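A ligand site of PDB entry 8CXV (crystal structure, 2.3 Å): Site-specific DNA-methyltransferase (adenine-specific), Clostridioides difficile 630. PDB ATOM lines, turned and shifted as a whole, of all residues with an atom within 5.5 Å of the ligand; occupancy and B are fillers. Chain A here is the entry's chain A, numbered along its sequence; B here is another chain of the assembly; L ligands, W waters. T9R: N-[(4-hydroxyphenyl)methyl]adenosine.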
ATOM      1  N   GLY A  29      24.152  27.557 -10.229  1.00  0.00           N
ATOM      2  CA  GLY A  29      24.926  27.739 -11.443  1.00  0.00           C
ATOM      3  C   GLY A  29      24.863  29.142 -12.017  1.00  0.00           C
ATOM      4  O   GLY A  29      25.461  29.433 -13.054  1.00  0.00           O
ATOM      5  N   ILE A  30      24.144  30.029 -11.321  1.00  0.00           N
ATOM      6  CA  ILE A  30      23.963  31.411 -11.735  1.00  0.00           C
ATOM      7  C   ILE A  30      24.586  32.318 -10.681  1.00  0.00           C
ATOM      8  O   ILE A  30      24.267  32.207  -9.497  1.00  0.00           O
ATOM      9  CB  ILE A  30      22.472  31.767 -11.944  1.00  0.00           C
ATOM     10  N   TYR A  31      25.477  33.220 -11.123  1.00  0.00           N
ATOM     11  CA  TYR A  31      26.212  34.104 -10.236  1.00  0.00           C
ATOM     12  C   TYR A  31      25.847  35.561 -10.533  1.00  0.00           C
ATOM     13  O   TYR A  31      25.717  35.950 -11.696  1.00  0.00           O
ATOM     14  CB  TYR A  31      27.726  33.905 -10.405  1.00  0.00           C
ATOM     15  CG  TYR A  31      28.191  32.512 -10.062  1.00  0.00           C
ATOM     16  CD1 TYR A  31      28.214  31.508 -11.033  1.00  0.00           C
ATOM     17  CD2 TYR A  31      28.613  32.186  -8.779  1.00  0.00           C
ATOM     18  CE1 TYR A  31      28.644  30.227 -10.724  1.00  0.00           C
ATOM     19  CE2 TYR A  31      29.042  30.914  -8.473  1.00  0.00           C
ATOM     20  CZ  TYR A  31      29.053  29.940  -9.443  1.00  0.00           C
ATOM     21  OH  TYR A  31      29.480  28.671  -9.124  1.00  0.00           O
ATOM     22  N   ILE A  62      27.131  36.409 -23.967  1.00  0.00           N
ATOM     23  CA  ILE A  62      26.984  34.989 -24.290  1.00  0.00           C
ATOM     24  C   ILE A  62      26.824  34.126 -23.056  1.00  0.00           C
ATOM     25  O   ILE A  62      26.754  32.893 -23.186  1.00  0.00           O
ATOM     26  CB  ILE A  62      28.183  34.474 -25.116  1.00  0.00           C
ATOM     27  CG1 ILE A  62      29.505  34.714 -24.396  1.00  0.00           C
ATOM     28  CG2 ILE A  62      28.207  35.115 -26.488  1.00  0.00           C
ATOM     29  CD1 ILE A  62      30.692  34.177 -25.169  1.00  0.00           C
ATOM     30  N   SER A  63      26.787  34.712 -21.866  1.00  0.00           N
ATOM     31  CA  SER A  63      26.395  34.012 -20.649  1.00  0.00           C
ATOM     32  C   SER A  63      25.483  34.930 -19.844  1.00  0.00           C
ATOM     33  O   SER A  63      25.679  35.173 -18.658  1.00  0.00           O
ATOM     34  CB  SER A  63      27.609  33.557 -19.837  1.00  0.00           C
ATOM     35  OG  SER A  63      28.524  34.623 -19.637  1.00  0.00           O
ATOM     36  N   CYS A  64      24.461  35.479 -20.522  1.00  0.00           N
ATOM     37  CA  CYS A  64      23.671  36.588 -19.998  1.00  0.00           C
ATOM     38  C   CYS A  64      22.920  36.250 -18.713  1.00  0.00           C
ATOM     39  O   CYS A  64      22.584  37.168 -17.956  1.00  0.00           O
ATOM     40  CB  CYS A  64      22.694  37.068 -21.063  1.00  0.00           C
ATOM     41  SG  CYS A  64      21.518  35.806 -21.586  1.00  0.00           S
ATOM     42  N   GLY A  65      22.644  34.970 -18.464  1.00  0.00           N
ATOM     43  CA  GLY A  65      21.921  34.608 -17.257  1.00  0.00           C
ATOM     44  C   GLY A  65      20.546  35.244 -17.241  1.00  0.00           C
ATOM     45  O   GLY A  65      19.793  35.165 -18.211  1.00  0.00           O
ATOM     46  N   ALA A 114      22.751  35.013 -24.875  1.00  0.00           N
ATOM     47  CA  ALA A 114      22.802  33.560 -24.949  1.00  0.00           C
ATOM     48  C   ALA A 114      23.107  32.981 -23.575  1.00  0.00           C
ATOM     49  O   ALA A 114      23.939  33.534 -22.841  1.00  0.00           O
ATOM     50  CB  ALA A 114      23.852  33.078 -25.958  1.00  0.00           C
ATOM     51  N   ASP A 115      22.436  31.890 -23.229  1.00  0.00           N
ATOM     52  CA  ASP A 115      22.723  31.200 -21.974  1.00  0.00           C
ATOM     53  C   ASP A 115      22.196  29.773 -22.071  1.00  0.00           C
ATOM     54  O   ASP A 115      21.213  29.500 -22.753  1.00  0.00           O
ATOM     55  CB  ASP A 115      22.109  31.922 -20.777  1.00  0.00           C
ATOM     56  CG  ASP A 115      22.755  31.518 -19.458  1.00  0.00           C
ATOM     57  OD1 ASP A 115      22.575  30.361 -19.036  1.00  0.00           O
ATOM     58  OD2 ASP A 115      23.459  32.366 -18.861  1.00  0.00           O
ATOM     59  N   ILE A 116      22.871  28.869 -21.355  1.00  0.00           N
ATOM     60  CA  ILE A 116      22.475  27.464 -21.377  1.00  0.00           C
ATOM     61  C   ILE A 116      21.237  27.210 -20.513  1.00  0.00           C
ATOM     62  O   ILE A 116      20.536  26.218 -20.730  1.00  0.00           O
ATOM     63  CB  ILE A 116      23.654  26.586 -20.923  1.00  0.00           C
ATOM     64  CG1 ILE A 116      23.404  25.108 -21.265  1.00  0.00           C
ATOM     65  CG2 ILE A 116      23.932  26.760 -19.441  1.00  0.00           C
ATOM     66  CD1 ILE A 116      23.330  24.818 -22.736  1.00  0.00           C
ATOM     67  N   ASP A 117      20.947  28.094 -19.560  1.00  0.00           N
ATOM     68  CA  ASP A 117      19.842  27.903 -18.622  1.00  0.00           C
ATOM     69  C   ASP A 117      18.548  28.440 -19.245  1.00  0.00           C
ATOM     70  O   ASP A 117      18.423  29.643 -19.475  1.00  0.00           O
ATOM     71  CB  ASP A 117      20.138  28.602 -17.293  1.00  0.00           C
ATOM     72  CG  ASP A 117      19.022  28.426 -16.287  1.00  0.00           C
ATOM     73  OD1 ASP A 117      18.131  27.587 -16.499  1.00  0.00           O
ATOM     74  OD2 ASP A 117      19.041  29.158 -15.262  1.00  0.00           O
ATOM     75  N   CYS A 149      21.242  28.033 -25.512  1.00  0.00           N
ATOM     76  CA  CYS A 149      22.163  27.167 -26.224  1.00  0.00           C
ATOM     77  C   CYS A 149      23.504  27.184 -25.501  1.00  0.00           C
ATOM     78  O   CYS A 149      23.703  27.925 -24.538  1.00  0.00           O
ATOM     79  CB  CYS A 149      22.355  27.626 -27.679  1.00  0.00           C
ATOM     80  SG  CYS A 149      23.273  29.178 -27.802  1.00  0.00           S
ATOM     81  N   ASP A 150      24.420  26.347 -25.986  1.00  0.00           N
ATOM     82  CA  ASP A 150      25.820  26.375 -25.569  1.00  0.00           C
ATOM     83  C   ASP A 150      26.534  27.385 -26.454  1.00  0.00           C
ATOM     84  O   ASP A 150      26.692  27.159 -27.668  1.00  0.00           O
ATOM     85  CB  ASP A 150      26.434  24.985 -25.677  1.00  0.00           C
ATOM     86  CG  ASP A 150      27.891  24.945 -25.230  1.00  0.00           C
ATOM     87  OD1 ASP A 150      28.459  25.997 -24.892  1.00  0.00           O
ATOM     88  OD2 ASP A 150      28.470  23.841 -25.233  1.00  0.00           O
ATOM     89  N   SER A 151      26.983  28.489 -25.860  1.00  0.00           N
ATOM     90  CA  SER A 151      27.612  29.550 -26.645  1.00  0.00           C
ATOM     91  C   SER A 151      28.901  29.103 -27.303  1.00  0.00           C
ATOM     92  O   SER A 151      29.334  29.717 -28.277  1.00  0.00           O
ATOM     93  CB  SER A 151      27.876  30.769 -25.753  1.00  0.00           C
ATOM     94  OG  SER A 151      26.666  31.320 -25.278  1.00  0.00           O
ATOM     95  N   LEU A 152      29.531  28.047 -26.789  1.00  0.00           N
ATOM     96  CA  LEU A 152      30.759  27.532 -27.392  1.00  0.00           C
ATOM     97  C   LEU A 152      30.500  26.628 -28.594  1.00  0.00           C
ATOM     98  O   LEU A 152      31.446  26.319 -29.319  1.00  0.00           O
ATOM     99  CB  LEU A 152      31.578  26.781 -26.342  1.00  0.00           C
ATOM    100  CG  LEU A 152      31.974  27.631 -25.136  1.00  0.00           C
ATOM    101  CD1 LEU A 152      32.897  26.859 -24.196  1.00  0.00           C
ATOM    102  CD2 LEU A 152      32.617  28.934 -25.580  1.00  0.00           C
ATOM    103  N   ASN A 166      29.792  38.150 -17.772  1.00  0.00           N
ATOM    104  CA  ASN A 166      30.539  37.363 -16.798  1.00  0.00           C
ATOM    105  C   ASN A 166      30.466  35.897 -17.188  1.00  0.00           C
ATOM    106  O   ASN A 166      29.427  35.240 -16.957  1.00  0.00           O
ATOM    107  CB  ASN A 166      29.975  37.590 -15.392  1.00  0.00           C
ATOM    108  CG  ASN A 166      30.697  36.792 -14.318  1.00  0.00           C
ATOM    109  OD1 ASN A 166      31.818  36.328 -14.532  1.00  0.00           O
ATOM    110  ND2 ASN A 166      30.063  36.644 -13.169  1.00  0.00           N
ATOM    111  N   PRO A 167      31.513  35.331 -17.780  1.00  0.00           N
ATOM    112  CA  PRO A 167      31.446  33.948 -18.266  1.00  0.00           C
ATOM    113  C   PRO A 167      31.467  32.954 -17.116  1.00  0.00           C
ATOM    114  O   PRO A 167      31.764  33.325 -15.969  1.00  0.00           O
ATOM    115  CB  PRO A 167      32.718  33.818 -19.113  1.00  0.00           C
ATOM    116  CG  PRO A 167      33.675  34.776 -18.484  1.00  0.00           C
ATOM    117  CD  PRO A 167      32.820  35.954 -18.036  1.00  0.00           C
ATOM    118  N   PRO A 168      31.114  31.699 -17.373  1.00  0.00           N
ATOM    119  CA  PRO A 168      31.278  30.668 -16.332  1.00  0.00           C
ATOM    120  C   PRO A 168      32.738  30.321 -16.115  1.00  0.00           C
ATOM    121  O   PRO A 168      33.534  30.283 -17.070  1.00  0.00           O
ATOM    122  CB  PRO A 168      30.499  29.479 -16.894  1.00  0.00           C
ATOM    123  CG  PRO A 168      30.524  29.683 -18.376  1.00  0.00           C
ATOM    124  CD  PRO A 168      30.446  31.167 -18.574  1.00  0.00           C
ATOM    125  N   ILE A 170      34.874  27.235 -14.801  1.00  0.00           N
ATOM    126  CA  ILE A 170      34.868  25.823 -14.418  1.00  0.00           C
ATOM    127  C   ILE A 170      36.260  25.262 -14.665  1.00  0.00           C
ATOM    128  O   ILE A 170      36.735  25.258 -15.801  1.00  0.00           O
ATOM    129  CB  ILE A 170      33.813  25.007 -15.186  1.00  0.00           C
ATOM    130  CG1 ILE A 170      32.430  25.655 -15.064  1.00  0.00           C
ATOM    131  CG2 ILE A 170      33.771  23.579 -14.667  1.00  0.00           C
ATOM    132  CD1 ILE A 170      31.320  24.917 -15.776  1.00  0.00           C
ATOM    133  N   LEU A 175      34.787  20.014 -14.476  1.00  0.00           N
ATOM    134  CA  LEU A 175      34.304  19.972 -15.855  1.00  0.00           C
ATOM    135  C   LEU A 175      34.194  18.517 -16.312  1.00  0.00           C
ATOM    136  O   LEU A 175      35.074  17.710 -16.028  1.00  0.00           O
ATOM    137  CB  LEU A 175      35.239  20.751 -16.784  1.00  0.00           C
ATOM    138  CG  LEU A 175      34.688  21.223 -18.131  1.00  0.00           C
ATOM    139  CD1 LEU A 175      33.389  21.986 -17.954  1.00  0.00           C
ATOM    140  CD2 LEU A 175      35.723  22.096 -18.830  1.00  0.00           C
ATOM    141  N   TYR A 179      32.813  16.738 -22.095  1.00  0.00           N
ATOM    142  CA  TYR A 179      32.890  18.112 -22.598  1.00  0.00           C
ATOM    143  C   TYR A 179      34.334  18.555 -22.811  1.00  0.00           C
ATOM    144  O   TYR A 179      34.611  19.312 -23.751  1.00  0.00           O
ATOM    145  CB  TYR A 179      32.179  19.057 -21.643  1.00  0.00           C
ATOM    146  CG  TYR A 179      31.816  20.392 -22.265  1.00  0.00           C
ATOM    147  CD1 TYR A 179      30.648  20.528 -23.000  1.00  0.00           C
ATOM    148  CD2 TYR A 179      32.631  21.495 -22.117  1.00  0.00           C
ATOM    149  CE1 TYR A 179      30.298  21.740 -23.580  1.00  0.00           C
ATOM    150  CE2 TYR A 179      32.301  22.711 -22.689  1.00  0.00           C
ATOM    151  CZ  TYR A 179      31.136  22.828 -23.419  1.00  0.00           C
ATOM    152  OH  TYR A 179      30.794  24.022 -23.988  1.00  0.00           O
ATOM    153  N   LEU A 197      37.424  26.692 -18.263  1.00  0.00           N
ATOM    154  CA  LEU A 197      36.383  26.913 -19.250  1.00  0.00           C
ATOM    155  C   LEU A 197      36.328  28.362 -19.716  1.00  0.00           C
ATOM    156  O   LEU A 197      36.073  28.640 -20.890  1.00  0.00           O
ATOM    157  CB  LEU A 197      35.027  26.496 -18.686  1.00  0.00           C
ATOM    158  CG  LEU A 197      33.808  26.716 -19.576  1.00  0.00           C
ATOM    159  CD1 LEU A 197      33.853  25.816 -20.790  1.00  0.00           C
ATOM    160  CD2 LEU A 197      32.525  26.500 -18.792  1.00  0.00           C
ATOM    161  N   PHE A 201      35.709  31.029 -23.474  1.00  0.00           N
ATOM    162  CA  PHE A 201      34.822  32.169 -23.650  1.00  0.00           C
ATOM    163  C   PHE A 201      35.605  33.399 -24.087  1.00  0.00           C
ATOM    164  O   PHE A 201      35.112  34.189 -24.905  1.00  0.00           O
ATOM    165  CB  PHE A 201      34.038  32.433 -22.373  1.00  0.00           C
ATOM    166  CG  PHE A 201      32.810  31.578 -22.234  1.00  0.00           C
ATOM    167  CD1 PHE A 201      32.905  30.254 -21.838  1.00  0.00           C
ATOM    168  CD2 PHE A 201      31.557  32.099 -22.533  1.00  0.00           C
ATOM    169  CE1 PHE A 201      31.785  29.468 -21.725  1.00  0.00           C
ATOM    170  CE2 PHE A 201      30.424  31.311 -22.422  1.00  0.00           C
ATOM    171  CZ  PHE A 201      30.538  29.991 -22.016  1.00  0.00           C
ATOM    172  P    DA B   8      37.739  26.727  -8.534  1.00  0.00           P
ATOM    173  OP1  DA B   8      37.014  25.674  -7.795  1.00  0.00           O
ATOM    174  OP2  DA B   8      37.956  26.600  -9.992  1.00  0.00           O
ATOM    175  O5'  DA B   8      37.042  28.135  -8.253  1.00  0.00           O
ATOM    176  C5'  DA B   8      35.975  28.576  -9.069  1.00  0.00           C
ATOM    177  C4'  DA B   8      35.067  29.482  -8.275  1.00  0.00           C
ATOM    178  O4'  DA B   8      34.463  30.473  -9.151  1.00  0.00           O
ATOM    179  C3'  DA B   8      33.911  28.779  -7.579  1.00  0.00           C
ATOM    180  O3'  DA B   8      33.714  29.354  -6.302  1.00  0.00           O
ATOM    181  C2'  DA B   8      32.730  29.068  -8.506  1.00  0.00           C
ATOM    182  C1'  DA B   8      33.081  30.480  -8.945  1.00  0.00           C
ATOM    183  N9   DA B   8      32.440  30.890 -10.191  1.00  0.00           N
ATOM    184  C8   DA B   8      32.182  30.124 -11.282  1.00  0.00           C
ATOM    185  N7   DA B   8      31.609  30.775 -12.268  1.00  0.00           N
ATOM    186  C5   DA B   8      31.482  32.061 -11.785  1.00  0.00           C
ATOM    187  C6   DA B   8      30.955  33.243 -12.352  1.00  0.00           C
ATOM    188  N6   DA B   8      30.429  33.301 -13.576  1.00  0.00           N
ATOM    189  N1   DA B   8      30.986  34.360 -11.600  1.00  0.00           N
ATOM    190  C2   DA B   8      31.503  34.302 -10.369  1.00  0.00           C
ATOM    191  N3   DA B   8      32.037  33.250  -9.733  1.00  0.00           N
ATOM    192  C4   DA B   8      31.991  32.157 -10.507  1.00  0.00           C
HETATM  193  C12 T9R L   1      27.857  22.120 -20.499  1.00  0.00           C
HETATM  194  O1  T9R L   1      26.898  31.143 -17.788  1.00  0.00           O
HETATM  195  C13 T9R L   1      29.127  22.465 -20.071  1.00  0.00           C
HETATM  196  C14 T9R L   1      29.648  23.708 -20.391  1.00  0.00           C
HETATM  197  C15 T9R L   1      27.643  31.837 -15.608  1.00  0.00           C
HETATM  198  C16 T9R L   1      25.278  29.718 -16.874  1.00  0.00           C
HETATM  199  O2  T9R L   1      27.330  20.909 -20.172  1.00  0.00           O
HETATM  200  O3  T9R L   1      27.360  32.692 -14.509  1.00  0.00           O
HETATM  201  O   T9R L   1      24.055  31.759 -16.276  1.00  0.00           O
HETATM  202  C7  T9R L   1      27.764  27.693 -21.932  1.00  0.00           C
HETATM  203  C8  T9R L   1      29.489  25.977 -21.474  1.00  0.00           C
HETATM  204  C9  T9R L   1      28.920  24.617 -21.146  1.00  0.00           C
HETATM  205  C10 T9R L   1      27.643  24.262 -21.566  1.00  0.00           C
HETATM  206  C11 T9R L   1      27.106  23.027 -21.250  1.00  0.00           C
HETATM  207  N4  T9R L   1      28.645  26.761 -22.360  1.00  0.00           N
HETATM  208  N   T9R L   1      26.598  29.142 -18.938  1.00  0.00           N
HETATM  209  C   T9R L   1      25.251  31.017 -16.058  1.00  0.00           C
HETATM  210  N1  T9R L   1      27.918  27.373 -19.386  1.00  0.00           N
HETATM  211  C1  T9R L   1      26.474  31.781 -16.566  1.00  0.00           C
HETATM  212  N2  T9R L   1      26.079  29.828 -21.206  1.00  0.00           N
HETATM  213  C2  T9R L   1      25.925  30.185 -18.172  1.00  0.00           C
HETATM  214  C3  T9R L   1      27.344  28.103 -18.454  1.00  0.00           C
HETATM  215  C4  T9R L   1      27.507  27.970 -20.569  1.00  0.00           C
HETATM  216  C5  T9R L   1      26.675  29.049 -20.301  1.00  0.00           C
HETATM  217  C6  T9R L   1      26.365  29.456 -22.458  1.00  0.00           C
HETATM  218  N3  T9R L   1      27.159  28.455 -22.864  1.00  0.00           N
HETATM  219  O4  T9R L   1      23.963  29.248 -17.139  1.00  0.00           O
HETATM  220  O   HOH W   1      27.627  24.681 -17.246  1.00  0.00           O
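A nitrogen (N4) of the ligand sits at hydrogen-bond distance from the side-chain carboxylate of Asp 150 (2.7 Å). The backbone NH (N) of Ser 151 sits at hydrogen-bond distance from a nitrogen (N3) of the ligand, 3.0 Å away. O4 of the ligand sits at hydrogen-bond distance from OD1 of Asp 115 (2.6 Å). N6 of DA 8 of chain B lies within hydrogen-bond range of O3 of the ligand (3.3 Å). N2 of the ligand sits at hydrogen-bond distance from N of Ile 116, at 3.4 Å.
The backbone NH (N) of Ser 63 is in hydrogen-bond range of the backbone carbonyl oxygen (O) of Ala 114, at 3.2 Å. The side-chain carboxylate of Asp 115 is in hydrogen-bond range of the backbone NH of Asp 117, 2.8 Å away. N1 of DA 8 of chain B is in hydrogen-bond range of the side-chain amide nitrogen (ND2) of Asn 166, 2.9 Å away. N of Cys 149 is in hydrogen-bond range of O of Asp 115 (3.1 Å). The side-chain carboxylate (OD1) of Asp 150 is in hydrogen-bond range of the backbone NH (N) of Leu 152 (3.0 Å). N6 of DA 8 of chain B sits close to the backbone carbonyl oxygen (O) of Pro 167 (2.7 Å). N of Ile 116 lies close to O of Cys 149 (3.4 Å). The backbone NH (N) of Gly 65 is in hydrogen-bond range of the side-chain carboxylate (OD2) of Asp 115 (2.8 Å).
Residues that only touch the ligand: Gly 29 (3.4 Å), Tyr 31 (3.8 Å), Ile 62 (3.5 Å), Ser 63 (3.2 Å), Gly 65 (3.7 Å), Asp 117 (3.9 Å), Cys 149 (3.7 Å), Pro 168 (3.6 Å), Tyr 179 (3.4 Å) and Phe 201 (3.6 Å). 15 residues have an atom within 4 Å of the ligand: Gly 29, Tyr 31, Ile 62, Ser 63, Gly 65, Asp 115, Ile 116, Asp 117, Cys 149, Asp 150, Ser 151, Pro 168, Tyr 179, Phe 201 and DA 8 of chain B. The nearest printed residue that does not touch the ligand is Asn 166 (4.1 Å).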
